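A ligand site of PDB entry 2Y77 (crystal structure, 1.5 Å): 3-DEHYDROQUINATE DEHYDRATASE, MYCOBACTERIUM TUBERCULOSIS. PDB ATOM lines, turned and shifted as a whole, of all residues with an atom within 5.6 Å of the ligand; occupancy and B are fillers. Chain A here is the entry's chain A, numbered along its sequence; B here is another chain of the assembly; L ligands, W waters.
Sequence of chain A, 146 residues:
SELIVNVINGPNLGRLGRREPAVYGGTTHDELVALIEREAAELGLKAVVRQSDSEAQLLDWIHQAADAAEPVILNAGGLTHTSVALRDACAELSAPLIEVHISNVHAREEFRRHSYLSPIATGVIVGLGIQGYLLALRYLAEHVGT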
ATOM      1  N   PRO A  11     -32.186 -27.839  -9.417  1.00  0.00           N
ATOM      2  CA  PRO A  11     -30.937 -28.346  -9.955  1.00  0.00           C
ATOM      3  C   PRO A  11     -29.918 -28.801  -8.917  1.00  0.00           C
ATOM      4  O   PRO A  11     -29.761 -28.159  -7.869  1.00  0.00           O
ATOM      5  CB  PRO A  11     -30.381 -27.167 -10.748  1.00  0.00           C
ATOM      6  CG  PRO A  11     -31.521 -26.323 -11.043  1.00  0.00           C
ATOM      7  CD  PRO A  11     -32.612 -26.600 -10.078  1.00  0.00           C
ATOM      8  N   ASN A  12     -29.263 -29.908  -9.243  1.00  0.00           N
ATOM      9  CA  ASN A  12     -28.203 -30.507  -8.440  1.00  0.00           C
ATOM     10  C   ASN A  12     -28.651 -31.290  -7.205  1.00  0.00           C
ATOM     11  O   ASN A  12     -27.871 -32.044  -6.638  1.00  0.00           O
ATOM     12  CB  ASN A  12     -27.133 -29.464  -8.069  1.00  0.00           C
ATOM     13  CG  ASN A  12     -26.509 -28.789  -9.292  1.00  0.00           C
ATOM     14  OD1 ASN A  12     -26.463 -27.546  -9.404  1.00  0.00           O
ATOM     15  ND2 ASN A  12     -26.050 -29.599 -10.228  1.00  0.00           N
ATOM     16  N   LEU A  13     -29.921 -31.177  -6.814  1.00  0.00           N
ATOM     17  CA  LEU A  13     -30.415 -31.890  -5.636  1.00  0.00           C
ATOM     18  C   LEU A  13     -30.423 -33.409  -5.847  1.00  0.00           C
ATOM     19  O   LEU A  13     -30.340 -34.161  -4.892  1.00  0.00           O
ATOM     20  CB  LEU A  13     -31.793 -31.403  -5.209  1.00  0.00           C
ATOM     21  CG  LEU A  13     -31.863 -30.186  -4.270  1.00  0.00           C
ATOM     22  CD1 LEU A  13     -31.297 -30.519  -2.867  1.00  0.00           C
ATOM     23  CD2 LEU A  13     -31.233 -28.959  -4.854  1.00  0.00           C
ATOM     24  N   ARG A  15     -28.005 -34.963  -6.875  1.00  0.00           N
ATOM     25  CA  ARG A  15     -26.623 -35.355  -6.558  1.00  0.00           C
ATOM     26  C   ARG A  15     -26.366 -35.510  -5.052  1.00  0.00           C
ATOM     27  O   ARG A  15     -25.254 -35.814  -4.653  1.00  0.00           O
ATOM     28  CB  ARG A  15     -25.633 -34.327  -7.128  1.00  0.00           C
ATOM     29  CG  ARG A  15     -25.792 -34.010  -8.598  1.00  0.00           C
ATOM     30  CD  ARG A  15     -25.391 -35.175  -9.461  1.00  0.00           C
ATOM     31  NE  ARG A  15     -23.984 -35.477  -9.230  1.00  0.00           N
ATOM     32  CZ  ARG A  15     -23.380 -36.594  -9.618  1.00  0.00           C
ATOM     33  NH1 ARG A  15     -24.042 -37.523 -10.290  1.00  0.00           N
ATOM     34  NH2 ARG A  15     -22.090 -36.765  -9.347  1.00  0.00           N
ATOM     35  N   LEU A  16     -27.380 -35.294  -4.214  1.00  0.00           N
ATOM     36  CA  LEU A  16     -27.233 -35.469  -2.780  1.00  0.00           C
ATOM     37  C   LEU A  16     -26.616 -36.823  -2.463  1.00  0.00           C
ATOM     38  O   LEU A  16     -27.009 -37.827  -3.047  1.00  0.00           O
ATOM     39  CB  LEU A  16     -28.592 -35.388  -2.100  1.00  0.00           C
ATOM     40  CG  LEU A  16     -29.142 -34.010  -1.749  1.00  0.00           C
ATOM     41  CD1 LEU A  16     -30.598 -34.167  -1.372  1.00  0.00           C
ATOM     42  CD2 LEU A  16     -28.331 -33.356  -0.620  1.00  0.00           C
ATOM     43  N   GLY A  17     -25.640 -36.836  -1.557  1.00  0.00           N
ATOM     44  CA  GLY A  17     -25.071 -38.087  -1.055  1.00  0.00           C
ATOM     45  C   GLY A  17     -24.058 -38.763  -1.956  1.00  0.00           C
ATOM     46  O   GLY A  17     -23.351 -39.668  -1.508  1.00  0.00           O
ATOM     47  N   ASN A  75     -37.038 -26.243  -2.687  1.00  0.00           N
ATOM     48  CA  ASN A  75     -35.603 -25.996  -2.665  1.00  0.00           C
ATOM     49  C   ASN A  75     -35.144 -25.901  -4.107  1.00  0.00           C
ATOM     50  O   ASN A  75     -34.946 -26.904  -4.774  1.00  0.00           O
ATOM     51  CB  ASN A  75     -34.852 -27.099  -1.926  1.00  0.00           C
ATOM     52  CG  ASN A  75     -33.373 -26.809  -1.835  1.00  0.00           C
ATOM     53  OD1 ASN A  75     -32.878 -25.894  -2.498  1.00  0.00           O
ATOM     54  ND2 ASN A  75     -32.658 -27.592  -1.016  1.00  0.00           N
ATOM     55  N   ALA A  76     -35.034 -24.668  -4.596  1.00  0.00           N
ATOM     56  CA  ALA A  76     -34.794 -24.427  -6.010  1.00  0.00           C
ATOM     57  C   ALA A  76     -33.324 -24.531  -6.432  1.00  0.00           C
ATOM     58  O   ALA A  76     -32.997 -24.314  -7.591  1.00  0.00           O
ATOM     59  CB  ALA A  76     -35.376 -23.060  -6.420  1.00  0.00           C
ATOM     60  N   GLY A  77     -32.432 -24.864  -5.485  1.00  0.00           N
ATOM     61  CA  GLY A  77     -31.009 -24.933  -5.790  1.00  0.00           C
ATOM     62  C   GLY A  77     -30.530 -23.597  -6.342  1.00  0.00           C
ATOM     63  O   GLY A  77     -30.965 -22.541  -5.894  1.00  0.00           O
ATOM     64  N   GLY A  78     -29.668 -23.621  -7.348  1.00  0.00           N
ATOM     65  CA  GLY A  78     -29.100 -22.372  -7.872  1.00  0.00           C
ATOM     66  C   GLY A  78     -30.126 -21.403  -8.428  1.00  0.00           C
ATOM     67  O   GLY A  78     -29.898 -20.185  -8.454  1.00  0.00           O
ATOM     68  N   LEU A  79     -31.273 -21.925  -8.856  1.00  0.00           N
ATOM     69  CA  LEU A  79     -32.313 -21.085  -9.422  1.00  0.00           C
ATOM     70  C   LEU A  79     -32.908 -20.133  -8.384  1.00  0.00           C
ATOM     71  O   LEU A  79     -33.487 -19.122  -8.753  1.00  0.00           O
ATOM     72  CB  LEU A  79     -33.422 -21.909 -10.046  1.00  0.00           C
ATOM     73  CG  LEU A  79     -32.980 -22.841 -11.173  1.00  0.00           C
ATOM     74  CD1 LEU A  79     -34.164 -23.691 -11.635  1.00  0.00           C
ATOM     75  CD2 LEU A  79     -32.329 -22.095 -12.340  1.00  0.00           C
ATOM     76  N   THR A  80     -32.762 -20.466  -7.099  1.00  0.00           N
ATOM     77  CA  THR A  80     -33.163 -19.564  -6.025  1.00  0.00           C
ATOM     78  C   THR A  80     -32.656 -18.154  -6.240  1.00  0.00           C
ATOM     79  O   THR A  80     -33.360 -17.168  -5.987  1.00  0.00           O
ATOM     80  CB  THR A  80     -32.598 -20.051  -4.701  1.00  0.00           C
ATOM     81  OG1 THR A  80     -32.976 -21.408  -4.491  1.00  0.00           O
ATOM     82  CG2 THR A  80     -33.073 -19.187  -3.524  1.00  0.00           C
ATOM     83  N   HIS A  81     -31.409 -18.061  -6.702  1.00  0.00           N
ATOM     84  CA  HIS A  81     -30.709 -16.811  -6.764  1.00  0.00           C
ATOM     85  C   HIS A  81     -30.838 -16.105  -8.110  1.00  0.00           C
ATOM     86  O   HIS A  81     -30.440 -14.941  -8.232  1.00  0.00           O
ATOM     87  CB  HIS A  81     -29.230 -17.048  -6.423  1.00  0.00           C
ATOM     88  CG  HIS A  81     -29.056 -17.957  -5.256  1.00  0.00           C
ATOM     89  ND1 HIS A  81     -29.487 -17.625  -3.987  1.00  0.00           N
ATOM     90  CD2 HIS A  81     -28.597 -19.230  -5.166  1.00  0.00           C
ATOM     91  CE1 HIS A  81     -29.258 -18.637  -3.166  1.00  0.00           C
ATOM     92  NE2 HIS A  81     -28.713 -19.620  -3.856  1.00  0.00           N
ATOM     93  N   VAL A 100     -36.895 -23.785   1.302  1.00  0.00           N
ATOM     94  CA  VAL A 100     -35.949 -24.536   2.114  1.00  0.00           C
ATOM     95  C   VAL A 100     -34.590 -24.588   1.418  1.00  0.00           C
ATOM     96  O   VAL A 100     -34.507 -24.807   0.196  1.00  0.00           O
ATOM     97  CB  VAL A 100     -36.462 -25.991   2.379  1.00  0.00           C
ATOM     98  CG1 VAL A 100     -35.383 -26.880   3.007  1.00  0.00           C
ATOM     99  CG2 VAL A 100     -37.696 -25.956   3.247  1.00  0.00           C
ATOM    100  N   HIS A 101     -33.530 -24.384   2.202  1.00  0.00           N
ATOM    101  CA  HIS A 101     -32.164 -24.681   1.794  1.00  0.00           C
ATOM    102  C   HIS A 101     -31.504 -25.540   2.840  1.00  0.00           C
ATOM    103  O   HIS A 101     -31.647 -25.289   4.036  1.00  0.00           O
ATOM    104  CB  HIS A 101     -31.392 -23.405   1.546  1.00  0.00           C
ATOM    105  CG  HIS A 101     -32.002 -22.562   0.478  1.00  0.00           C
ATOM    106  ND1 HIS A 101     -31.954 -22.929  -0.845  1.00  0.00           N
ATOM    107  CD2 HIS A 101     -32.779 -21.454   0.544  1.00  0.00           C
ATOM    108  CE1 HIS A 101     -32.624 -22.040  -1.557  1.00  0.00           C
ATOM    109  NE2 HIS A 101     -33.134 -21.145  -0.742  1.00  0.00           N
ATOM    110  N   ILE A 102     -30.805 -26.576   2.396  1.00  0.00           N
ATOM    111  CA  ILE A 102     -30.132 -27.506   3.277  1.00  0.00           C
ATOM    112  C   ILE A 102     -28.976 -26.780   3.956  1.00  0.00           C
ATOM    113  O   ILE A 102     -28.803 -26.902   5.163  1.00  0.00           O
ATOM    114  CB  ILE A 102     -29.662 -28.717   2.446  1.00  0.00           C
ATOM    115  CG1 ILE A 102     -30.887 -29.536   2.037  1.00  0.00           C
ATOM    116  CG2 ILE A 102     -28.652 -29.567   3.240  1.00  0.00           C
ATOM    117  CD1 ILE A 102     -30.583 -30.604   1.027  1.00  0.00           C
ATOM    118  N   SER A 103     -28.197 -26.031   3.186  1.00  0.00           N
ATOM    119  CA  SER A 103     -27.058 -25.278   3.682  1.00  0.00           C
ATOM    120  C   SER A 103     -27.492 -23.911   4.187  1.00  0.00           C
ATOM    121  O   SER A 103     -28.582 -23.424   3.871  1.00  0.00           O
ATOM    122  CB  SER A 103     -25.991 -25.140   2.577  1.00  0.00           C
ATOM    123  OG  SER A 103     -26.340 -24.153   1.624  1.00  0.00           O
ATOM    124  N   ASN A 104     -26.632 -23.298   4.999  1.00  0.00           N
ATOM    125  CA  ASN A 104     -26.869 -21.918   5.391  1.00  0.00           C
ATOM    126  C   ASN A 104     -26.369 -21.008   4.283  1.00  0.00           C
ATOM    127  O   ASN A 104     -25.168 -20.705   4.199  1.00  0.00           O
ATOM    128  CB  ASN A 104     -26.185 -21.593   6.717  1.00  0.00           C
ATOM    129  CG  ASN A 104     -26.527 -20.196   7.186  1.00  0.00           C
ATOM    130  OD1 ASN A 104     -27.046 -19.386   6.424  1.00  0.00           O
ATOM    131  ND2 ASN A 104     -26.231 -19.899   8.463  1.00  0.00           N
ATOM    132  N   VAL A 105     -27.300 -20.582   3.428  1.00  0.00           N
ATOM    133  CA  VAL A 105     -26.955 -19.760   2.266  1.00  0.00           C
ATOM    134  C   VAL A 105     -26.419 -18.383   2.634  1.00  0.00           C
ATOM    135  O   VAL A 105     -25.919 -17.680   1.762  1.00  0.00           O
ATOM    136  CB  VAL A 105     -28.141 -19.592   1.309  1.00  0.00           C
ATOM    137  CG1 VAL A 105     -28.434 -20.924   0.626  1.00  0.00           C
ATOM    138  CG2 VAL A 105     -29.375 -19.033   2.028  1.00  0.00           C
ATOM    139  N   ARG A 108     -21.829 -18.185   3.022  1.00  0.00           N
ATOM    140  CA  ARG A 108     -20.759 -18.285   2.024  1.00  0.00           C
ATOM    141  C   ARG A 108     -20.808 -17.138   1.017  1.00  0.00           C
ATOM    142  O   ARG A 108     -20.717 -15.997   1.458  1.00  0.00           O
ATOM    143  CB  ARG A 108     -20.637 -19.673   1.407  1.00  0.00           C
ATOM    144  CG  ARG A 108     -21.888 -20.299   0.904  1.00  0.00           C
ATOM    145  CD  ARG A 108     -21.496 -21.691   0.385  1.00  0.00           C
ATOM    146  NE  ARG A 108     -22.562 -22.381  -0.301  1.00  0.00           N
ATOM    147  CZ  ARG A 108     -23.738 -22.663   0.239  1.00  0.00           C
ATOM    148  NH1 ARG A 108     -24.009 -22.275   1.473  1.00  0.00           N
ATOM    149  NH2 ARG A 108     -24.643 -23.312  -0.483  1.00  0.00           N
ATOM    150  N   ARG A 112     -25.339 -15.814  -2.855  1.00  0.00           N
ATOM    151  CA  ARG A 112     -26.312 -16.777  -2.291  1.00  0.00           C
ATOM    152  C   ARG A 112     -27.242 -16.170  -1.255  1.00  0.00           C
ATOM    153  O   ARG A 112     -28.212 -16.801  -0.850  1.00  0.00           O
ATOM    154  CB  ARG A 112     -25.626 -17.953  -1.625  1.00  0.00           C
ATOM    155  CG  ARG A 112     -25.018 -18.886  -2.578  1.00  0.00           C
ATOM    156  CD  ARG A 112     -24.538 -20.164  -1.928  1.00  0.00           C
ATOM    157  NE  ARG A 112     -23.451 -20.645  -2.743  1.00  0.00           N
ATOM    158  CZ  ARG A 112     -23.611 -21.319  -3.887  1.00  0.00           C
ATOM    159  NH1 ARG A 112     -24.814 -21.710  -4.306  1.00  0.00           N
ATOM    160  NH2 ARG A 112     -22.539 -21.649  -4.580  1.00  0.00           N
ATOM    161  N   TYR A 133     -36.729 -29.762   5.600  1.00  0.00           N
ATOM    162  CA  TYR A 133     -37.924 -30.221   4.891  1.00  0.00           C
ATOM    163  C   TYR A 133     -38.969 -30.743   5.864  1.00  0.00           C
ATOM    164  O   TYR A 133     -40.155 -30.489   5.696  1.00  0.00           O
ATOM    165  CB  TYR A 133     -37.601 -31.346   3.935  1.00  0.00           C
ATOM    166  CG  TYR A 133     -36.727 -30.958   2.757  1.00  0.00           C
ATOM    167  CD1 TYR A 133     -37.283 -30.491   1.580  1.00  0.00           C
ATOM    168  CD2 TYR A 133     -35.335 -31.099   2.812  1.00  0.00           C
ATOM    169  CE1 TYR A 133     -36.494 -30.169   0.491  1.00  0.00           C
ATOM    170  CE2 TYR A 133     -34.544 -30.785   1.735  1.00  0.00           C
ATOM    171  CZ  TYR A 133     -35.124 -30.327   0.583  1.00  0.00           C
ATOM    172  OH  TYR A 133     -34.336 -30.056  -0.503  1.00  0.00           O
ATOM    173  N   VAL B  84     -26.016 -19.923 -11.568  1.00  0.00           N
ATOM    174  CA  VAL B  84     -25.457 -20.484 -10.348  1.00  0.00           C
ATOM    175  C   VAL B  84     -25.590 -22.013 -10.375  1.00  0.00           C
ATOM    176  O   VAL B  84     -24.690 -22.712  -9.902  1.00  0.00           O
ATOM    177  CB  VAL B  84     -26.145 -19.903  -9.086  1.00  0.00           C
ATOM    178  CG1 VAL B  84     -25.729 -20.668  -7.841  1.00  0.00           C
ATOM    179  CG2 VAL B  84     -25.810 -18.413  -8.933  1.00  0.00           C
ATOM    180  N   ASP B  88     -22.529 -24.539  -9.626  1.00  0.00           N
ATOM    181  CA  ASP B  88     -22.605 -25.493  -8.531  1.00  0.00           C
ATOM    182  C   ASP B  88     -22.389 -26.942  -9.012  1.00  0.00           C
ATOM    183  O   ASP B  88     -21.726 -27.738  -8.326  1.00  0.00           O
ATOM    184  CB  ASP B  88     -23.939 -25.312  -7.795  1.00  0.00           C
ATOM    185  CG  ASP B  88     -23.957 -24.083  -6.894  1.00  0.00           C
ATOM    186  OD1 ASP B  88     -22.898 -23.439  -6.709  1.00  0.00           O
ATOM    187  OD2 ASP B  88     -25.013 -23.738  -6.373  1.00  0.00           O
HETATM  188  C1  LIG L   1     -27.647 -25.512  -3.852  1.00  0.00           C
HETATM  189  C2  LIG L   1     -27.212 -24.039  -4.012  1.00  0.00           C
HETATM  190  O1  LIG L   1     -27.319 -23.691  -5.407  1.00  0.00           O
HETATM  191  C3  LIG L   1     -28.070 -23.108  -3.148  1.00  0.00           C
HETATM  192  O2  LIG L   1     -27.420 -21.833  -3.047  1.00  0.00           O
HETATM  193  C4  LIG L   1     -28.188 -23.687  -1.743  1.00  0.00           C
HETATM  194  C5  LIG L   1     -28.958 -25.009  -1.778  1.00  0.00           C
HETATM  195  C6  LIG L   1     -29.210 -25.590  -0.395  1.00  0.00           C
HETATM  196  O3  LIG L   1     -30.171 -26.386  -0.290  1.00  0.00           O
HETATM  197  O4  LIG L   1     -28.455 -25.238   0.533  1.00  0.00           O
HETATM  198  O5  LIG L   1     -30.514 -24.642  -2.359  1.00  0.00           O
HETATM  199  C7  LIG L   1     -28.330 -26.018  -2.749  1.00  0.00           C
HETATM  200  C8  LIG L   1     -24.595 -28.415  -3.106  1.00  0.00           C
HETATM  201  C9  LIG L   1     -24.554 -29.711  -2.724  1.00  0.00           C
HETATM  202  C10 LIG L   1     -23.731 -30.312  -1.766  1.00  0.00           C
HETATM  203  C11 LIG L   1     -23.819 -31.671  -1.479  1.00  0.00           C
HETATM  204  C12 LIG L   1     -24.737 -32.449  -2.168  1.00  0.00           C
HETATM  205  C13 LIG L   1     -25.575 -31.877  -3.124  1.00  0.00           C
HETATM  206  C14 LIG L   1     -25.485 -30.526  -3.399  1.00  0.00           C
HETATM  207  S1  LIG L   1     -26.310 -29.529  -4.484  1.00  0.00           S
HETATM  208  C15 LIG L   1     -25.485 -28.124  -4.054  1.00  0.00           C
HETATM  209  C16 LIG L   1     -25.745 -26.826  -4.614  1.00  0.00           C
HETATM  210  O6  LIG L   1     -27.259 -26.398  -4.828  1.00  0.00           O
HETATM  211  C17 LIG L   1     -28.713 -27.506  -2.669  1.00  0.00           C
HETATM  212  C18 LIG L   1     -27.843 -28.213  -1.627  1.00  0.00           C
HETATM  213  C19 LIG L   1     -27.921 -29.483  -1.211  1.00  0.00           C
HETATM  214  C20 LIG L   1     -27.001 -29.828  -0.277  1.00  0.00           C
HETATM  215  C21 LIG L   1     -26.147 -28.866   0.100  1.00  0.00           C
HETATM  216  S2  LIG L   1     -26.554 -27.496  -0.797  1.00  0.00           S
HETATM  217  O   HOH W   1     -28.117 -25.941  -7.544  1.00  0.00           O
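The side-chain carboxylate (OD2) of Asp 88 of chain B lies within hydrogen-bond range of an oxygen (O1) of the ligand. N of Ile 102 sits at hydrogen-bond distance from O3 of the ligand, at 2.8 Å. An oxygen (O4) of the ligand sits at hydrogen-bond distance from the side-chain hydroxyl (OG) of Ser 103 (2.6 Å). NE2 of His 81 is in hydrogen-bond range of O2 of the ligand (2.7 Å). The backbone NH (N) of Gly 78 lies within hydrogen-bond range of an oxygen (O1) of the ligand (3.0 Å). The backbone NH of Ser 103 lies within hydrogen-bond range of an oxygen (O4) of the ligand, at 2.8 Å. O5 of the ligand sits at hydrogen-bond distance from ND1 of His 101. NH1 of Arg 112 sits at hydrogen-bond distance from O2 of the ligand, at 2.9 Å. OD1 of Asn 75 sits at hydrogen-bond distance from O5 of the ligand, 2.7 Å away.
The side-chain amide oxygen (OD1) of Asn 75 lies within hydrogen-bond range of the backbone NH (N) of Gly 77. The guanidinium group (NH1) of Arg 108 sits at hydrogen-bond distance from the backbone carbonyl oxygen (O) of Asn 104, at 3.4 Å. The side-chain carboxylate (OD1) of Asp 88 of chain B is in salt-bridge range of the guanidinium group (NH2) of Arg 112 (2.8 Å). OH of Tyr 133 sits at hydrogen-bond distance from ND2 of Asn 75 (3.0 Å). A ring nitrogen (ND1) of His 81 lies close to the backbone carbonyl oxygen of Arg 112, at 3.5 Å. O of Gly 77 is in hydrogen-bond range of OG1 of Thr 80. OD1 of Asn 75 lies close to O of Val 100 (3.3 Å). The guanidinium group of Arg 108 lies within hydrogen-bond range of the side-chain hydroxyl of Ser 103, at 2.8 Å.
The backbone carbonyl oxygen (O) of Asn 12 sits close to a sulfur (S1) of the ligand, at 3.7 Å. Leu 13 touches the ligand (CD2 to C17, 3.6 Å). Leu 16 touches the ligand. C of Gly 77 touches O1 of the ligand, at 3.3 Å. CG1 of Val 105 touches C4 of the ligand, at 3.6 Å. Arg 108 touches the ligand (NH2 to C4, 3.8 Å). Hydrophobic or aromatic side chains within 4 Å of the ligand: Leu 13, Leu 16, His 81, His 101, Ile 102 and Val 105. The nearest printed residue that does not touch the ligand is Arg 15 (4.2 Å).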
